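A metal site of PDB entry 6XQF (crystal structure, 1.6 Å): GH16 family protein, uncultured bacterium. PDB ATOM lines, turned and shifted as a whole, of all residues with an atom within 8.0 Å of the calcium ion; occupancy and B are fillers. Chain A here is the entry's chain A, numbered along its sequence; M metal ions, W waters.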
ATOM      1  N   ASP A  30      -1.767 -28.120   1.224  1.00  0.00           N
ATOM      2  CA  ASP A  30      -1.542 -27.630   2.607  1.00  0.00           C
ATOM      3  C   ASP A  30      -0.951 -26.250   2.406  1.00  0.00           C
ATOM      4  O   ASP A  30       0.231 -26.175   1.956  1.00  0.00           O
ATOM      5  CB  ASP A  30      -0.638 -28.502   3.472  1.00  0.00           C
ATOM      6  CG  ASP A  30      -0.887 -28.120   4.930  1.00  0.00           C
ATOM      7  OD1 ASP A  30      -1.395 -27.021   5.178  1.00  0.00           O
ATOM      8  OD2 ASP A  30      -0.600 -28.926   5.784  1.00  0.00           O
ATOM      9  N   GLU A  31      -1.734 -25.236   2.697  1.00  0.00           N
ATOM     10  CA  GLU A  31      -1.305 -23.827   2.601  1.00  0.00           C
ATOM     11  C   GLU A  31      -0.691 -23.416   3.928  1.00  0.00           C
ATOM     12  O   GLU A  31      -0.134 -22.310   3.947  1.00  0.00           O
ATOM     13  CB  GLU A  31      -2.503 -22.923   2.285  1.00  0.00           C
ATOM     14  CG  GLU A  31      -3.229 -23.329   0.997  1.00  0.00           C
ATOM     15  CD  GLU A  31      -2.495 -22.890  -0.265  1.00  0.00           C
ATOM     16  OE1 GLU A  31      -1.511 -22.107  -0.124  1.00  0.00           O
ATOM     17  OE2 GLU A  31      -2.947 -23.310  -1.362  1.00  0.00           O
ATOM     18  N   PHE A  32      -0.709 -24.262   4.959  1.00  0.00           N
ATOM     19  CA  PHE A  32      -0.115 -23.958   6.287  1.00  0.00           C
ATOM     20  C   PHE A  32      -0.763 -22.686   6.847  1.00  0.00           C
ATOM     21  O   PHE A  32      -0.156 -21.862   7.459  1.00  0.00           O
ATOM     22  CB  PHE A  32       1.417 -24.004   6.182  1.00  0.00           C
ATOM     23  CG  PHE A  32       1.937 -25.327   5.734  1.00  0.00           C
ATOM     24  CD1 PHE A  32       1.816 -26.450   6.546  1.00  0.00           C
ATOM     25  CD2 PHE A  32       2.566 -25.445   4.522  1.00  0.00           C
ATOM     26  CE1 PHE A  32       2.232 -27.694   6.112  1.00  0.00           C
ATOM     27  CE2 PHE A  32       3.011 -26.682   4.086  1.00  0.00           C
ATOM     28  CZ  PHE A  32       2.918 -27.787   4.922  1.00  0.00           C
ATOM     29  N   ASN A  33      -2.069 -22.635   6.632  1.00  0.00           N
ATOM     30  CA  ASN A  33      -2.917 -21.522   7.085  1.00  0.00           C
ATOM     31  C   ASN A  33      -3.103 -21.551   8.611  1.00  0.00           C
ATOM     32  O   ASN A  33      -3.430 -20.510   9.151  1.00  0.00           O
ATOM     33  CB  ASN A  33      -4.320 -21.590   6.476  1.00  0.00           C
ATOM     34  CG  ASN A  33      -4.369 -21.187   5.024  1.00  0.00           C
ATOM     35  OD1 ASN A  33      -3.411 -20.620   4.499  1.00  0.00           O
ATOM     36  ND2 ASN A  33      -5.485 -21.476   4.383  1.00  0.00           N
ATOM     37  N   THR A  34      -2.991 -22.699   9.273  1.00  0.00           N
ATOM     38  CA  THR A  34      -3.472 -22.834  10.672  1.00  0.00           C
ATOM     39  C   THR A  34      -2.298 -22.922  11.623  1.00  0.00           C
ATOM     40  O   THR A  34      -1.638 -23.939  11.694  1.00  0.00           O
ATOM     41  CB  THR A  34      -4.398 -24.035  10.813  1.00  0.00           C
ATOM     42  OG1 THR A  34      -5.436 -23.807   9.865  1.00  0.00           O
ATOM     43  CG2 THR A  34      -4.949 -24.225  12.202  1.00  0.00           C
ATOM     44  N   VAL A  72       3.738 -24.763  12.636  1.00  0.00           N
ATOM     45  CA  VAL A  72       3.185 -23.859  11.592  1.00  0.00           C
ATOM     46  C   VAL A  72       3.143 -22.474  12.219  1.00  0.00           C
ATOM     47  O   VAL A  72       2.562 -22.260  13.311  1.00  0.00           O
ATOM     48  CB  VAL A  72       1.846 -24.353  11.051  1.00  0.00           C
ATOM     49  CG1 VAL A  72       1.198 -23.335  10.106  1.00  0.00           C
ATOM     50  CG2 VAL A  72       1.925 -25.716  10.415  1.00  0.00           C
ATOM     51  N   GLU A  73       3.729 -21.510  11.533  1.00  0.00           N
ATOM     52  CA  GLU A  73       3.813 -20.108  11.956  1.00  0.00           C
ATOM     53  C   GLU A  73       3.772 -19.215  10.729  1.00  0.00           C
ATOM     54  O   GLU A  73       4.518 -19.514   9.761  1.00  0.00           O
ATOM     55  CB  GLU A  73       5.184 -19.730  12.512  1.00  0.00           C
ATOM     56  CG  GLU A  73       5.566 -20.350  13.815  1.00  0.00           C
ATOM     57  CD  GLU A  73       6.953 -19.930  14.298  1.00  0.00           C
ATOM     58  OE1 GLU A  73       7.733 -19.345  13.532  1.00  0.00           O
ATOM     59  OE2 GLU A  73       7.226 -20.161  15.393  1.00  0.00           O
ATOM     60  N   ASN A  74       2.910 -18.219  10.751  1.00  0.00           N
ATOM     61  CA  ASN A  74       2.896 -17.127   9.752  1.00  0.00           C
ATOM     62  C   ASN A  74       2.699 -17.722   8.358  1.00  0.00           C
ATOM     63  O   ASN A  74       3.340 -17.299   7.442  1.00  0.00           O
ATOM     64  CB  ASN A  74       4.143 -16.253   9.879  1.00  0.00           C
ATOM     65  CG  ASN A  74       4.245 -15.583  11.242  1.00  0.00           C
ATOM     66  OD1 ASN A  74       5.257 -15.815  11.925  1.00  0.00           O
ATOM     67  ND2 ASN A  74       3.212 -14.883  11.667  1.00  0.00           N
ATOM     68  N   GLY A  75       1.850 -18.713   8.218  1.00  0.00           N
ATOM     69  CA  GLY A  75       1.494 -19.255   6.894  1.00  0.00           C
ATOM     70  C   GLY A  75       2.532 -20.246   6.385  1.00  0.00           C
ATOM     71  O   GLY A  75       2.430 -20.623   5.237  1.00  0.00           O
ATOM     72  N   ASN A  76       3.517 -20.645   7.199  1.00  0.00           N
ATOM     73  CA  ASN A  76       4.566 -21.562   6.743  1.00  0.00           C
ATOM     74  C   ASN A  76       4.672 -22.737   7.706  1.00  0.00           C
ATOM     75  O   ASN A  76       4.571 -22.527   8.922  1.00  0.00           O
ATOM     76  CB  ASN A  76       5.964 -20.914   6.754  1.00  0.00           C
ATOM     77  CG  ASN A  76       6.121 -19.739   5.834  1.00  0.00           C
ATOM     78  OD1 ASN A  76       5.679 -19.812   4.671  1.00  0.00           O
ATOM     79  ND2 ASN A  76       6.720 -18.667   6.370  1.00  0.00           N
ATOM     80  N   LEU A  77       4.895 -23.904   7.149  1.00  0.00           N
ATOM     81  CA  LEU A  77       5.476 -25.038   7.904  1.00  0.00           C
ATOM     82  C   LEU A  77       6.905 -24.668   8.224  1.00  0.00           C
ATOM     83  O   LEU A  77       7.626 -24.227   7.335  1.00  0.00           O
ATOM     84  CB  LEU A  77       5.390 -26.343   7.116  1.00  0.00           C
ATOM     85  CG  LEU A  77       5.947 -27.548   7.871  1.00  0.00           C
ATOM     86  CD1 LEU A  77       4.966 -27.874   9.024  1.00  0.00           C
ATOM     87  CD2 LEU A  77       6.111 -28.690   6.887  1.00  0.00           C
ATOM     88  N   ARG A 118       6.476 -24.453  -2.363  1.00  0.00           N
ATOM     89  CA  ARG A 118       7.119 -23.150  -2.259  1.00  0.00           C
ATOM     90  C   ARG A 118       7.846 -23.098  -0.909  1.00  0.00           C
ATOM     91  O   ARG A 118       7.225 -23.252   0.172  1.00  0.00           O
ATOM     92  CB  ARG A 118       6.118 -22.022  -2.414  1.00  0.00           C
ATOM     93  CG  ARG A 118       6.786 -20.677  -2.235  1.00  0.00           C
ATOM     94  CD  ARG A 118       5.956 -19.531  -2.764  1.00  0.00           C
ATOM     95  NE  ARG A 118       6.671 -18.249  -2.836  1.00  0.00           N
ATOM     96  CZ  ARG A 118       6.628 -17.297  -1.898  1.00  0.00           C
ATOM     97  NH1 ARG A 118       5.974 -17.456  -0.754  1.00  0.00           N
ATOM     98  NH2 ARG A 118       7.344 -16.199  -2.048  1.00  0.00           N
ATOM     99  N   PHE A 191      12.167 -17.603  -0.901  1.00  0.00           N
ATOM    100  CA  PHE A 191      11.328 -18.700  -1.374  1.00  0.00           C
ATOM    101  C   PHE A 191      11.619 -18.997  -2.830  1.00  0.00           C
ATOM    102  O   PHE A 191      11.829 -18.094  -3.652  1.00  0.00           O
ATOM    103  CB  PHE A 191       9.863 -18.390  -1.130  1.00  0.00           C
ATOM    104  CG  PHE A 191       9.466 -18.550   0.307  1.00  0.00           C
ATOM    105  CD1 PHE A 191       9.494 -17.454   1.134  1.00  0.00           C
ATOM    106  CD2 PHE A 191       9.099 -19.763   0.814  1.00  0.00           C
ATOM    107  CE1 PHE A 191       9.098 -17.563   2.462  1.00  0.00           C
ATOM    108  CE2 PHE A 191       8.766 -19.887   2.152  1.00  0.00           C
ATOM    109  CZ  PHE A 191       8.754 -18.783   2.973  1.00  0.00           C
ATOM    110  N   VAL A 260       8.147 -23.824   4.620  1.00  0.00           N
ATOM    111  CA  VAL A 260       7.328 -24.234   3.463  1.00  0.00           C
ATOM    112  C   VAL A 260       6.060 -23.405   3.444  1.00  0.00           C
ATOM    113  O   VAL A 260       5.228 -23.550   4.371  1.00  0.00           O
ATOM    114  CB  VAL A 260       7.011 -25.728   3.463  1.00  0.00           C
ATOM    115  CG1 VAL A 260       6.292 -26.119   2.169  1.00  0.00           C
ATOM    116  CG2 VAL A 260       8.254 -26.591   3.716  1.00  0.00           C
ATOM    117  N   ASP A 261       5.869 -22.586   2.424  1.00  0.00           N
ATOM    118  CA  ASP A 261       4.675 -21.716   2.326  1.00  0.00           C
ATOM    119  C   ASP A 261       3.474 -22.593   1.992  1.00  0.00           C
ATOM    120  O   ASP A 261       2.334 -22.413   2.521  1.00  0.00           O
ATOM    121  CB  ASP A 261       4.902 -20.697   1.231  1.00  0.00           C
ATOM    122  CG  ASP A 261       3.789 -19.682   1.094  1.00  0.00           C
ATOM    123  OD1 ASP A 261       2.911 -19.608   1.964  1.00  0.00           O
ATOM    124  OD2 ASP A 261       3.849 -18.927   0.114  1.00  0.00           O
ATOM    125  N   TYR A 262       3.699 -23.511   1.048  1.00  0.00           N
ATOM    126  CA  TYR A 262       2.581 -24.378   0.666  1.00  0.00           C
ATOM    127  C   TYR A 262       3.089 -25.582  -0.063  1.00  0.00           C
ATOM    128  O   TYR A 262       4.183 -25.588  -0.628  1.00  0.00           O
ATOM    129  CB  TYR A 262       1.507 -23.687  -0.209  1.00  0.00           C
ATOM    130  CG  TYR A 262       2.003 -23.141  -1.524  1.00  0.00           C
ATOM    131  CD1 TYR A 262       2.338 -23.966  -2.578  1.00  0.00           C
ATOM    132  CD2 TYR A 262       2.180 -21.781  -1.671  1.00  0.00           C
ATOM    133  CE1 TYR A 262       2.828 -23.445  -3.772  1.00  0.00           C
ATOM    134  CE2 TYR A 262       2.619 -21.243  -2.892  1.00  0.00           C
ATOM    135  CZ  TYR A 262       2.988 -22.091  -3.933  1.00  0.00           C
ATOM    136  OH  TYR A 262       3.444 -21.615  -5.171  1.00  0.00           O
ATOM    137  N   VAL A 263       2.247 -26.605  -0.009  1.00  0.00           N
ATOM    138  CA  VAL A 263       2.316 -27.801  -0.855  1.00  0.00           C
ATOM    139  C   VAL A 263       1.005 -27.817  -1.655  1.00  0.00           C
ATOM    140  O   VAL A 263      -0.086 -27.823  -1.038  1.00  0.00           O
ATOM    141  CB  VAL A 263       2.470 -29.089  -0.056  1.00  0.00           C
ATOM    142  CG1 VAL A 263       2.289 -30.289  -0.974  1.00  0.00           C
ATOM    143  CG2 VAL A 263       3.771 -29.092   0.721  1.00  0.00           C
ATOM    144  N   ARG A 264       1.105 -27.748  -2.978  1.00  0.00           N
ATOM    145  CA  ARG A 264      -0.118 -27.868  -3.819  1.00  0.00           C
ATOM    146  C   ARG A 264       0.017 -29.016  -4.802  1.00  0.00           C
ATOM    147  O   ARG A 264       1.020 -29.091  -5.534  1.00  0.00           O
ATOM    148  CB  ARG A 264      -0.391 -26.575  -4.571  1.00  0.00           C
ATOM    149  CG  ARG A 264      -0.835 -25.439  -3.643  1.00  0.00           C
ATOM    150  CD  ARG A 264      -0.796 -24.103  -4.362  1.00  0.00           C
ATOM    151  NE  ARG A 264      -1.006 -23.008  -3.405  1.00  0.00           N
ATOM    152  CZ  ARG A 264      -0.711 -21.721  -3.630  1.00  0.00           C
ATOM    153  NH1 ARG A 264      -0.282 -21.306  -4.817  1.00  0.00           N
ATOM    154  NH2 ARG A 264      -0.935 -20.823  -2.699  1.00  0.00           N
HETATM  155 CA    CA M   1       1.157 -20.504   3.339  1.00  0.00          CA
HETATM  156  O   HOH W   1       1.396 -17.933   3.530  1.00  0.00           O
HETATM  157  O   HOH W   2      -0.875 -19.718   4.514  1.00  0.00           O
HETATM  158  O   HOH W   3      -0.048 -20.340   1.244  1.00  0.00           O
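OE2 of Glu 31 is in salt-bridge range of NE of Arg 264.
OD2 of Asp 261 is in salt-bridge range of NH1 of Arg 118 (2.7 Å).
The nearest printed residue that does not touch the calcium ion is Phe 32 (4.5 Å).
O of Gly 75 is bound to the calcium ion (2.3 Å).
O of Glu 31 is bound to the calcium ion, at 2.3 Å.
The backbone carbonyl oxygen (O) of Asp 261 binds the calcium ion (2.4 Å).
OD1 of Asp 261 is bound to the calcium ion.
Water W3 is bound to the calcium ion, 2.4 Å away.
Water W2 binds the calcium ion, 2.5 Å away.
Water W1 is bound to the calcium ion.
The calcium ion has seven donor atoms within binding distance.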
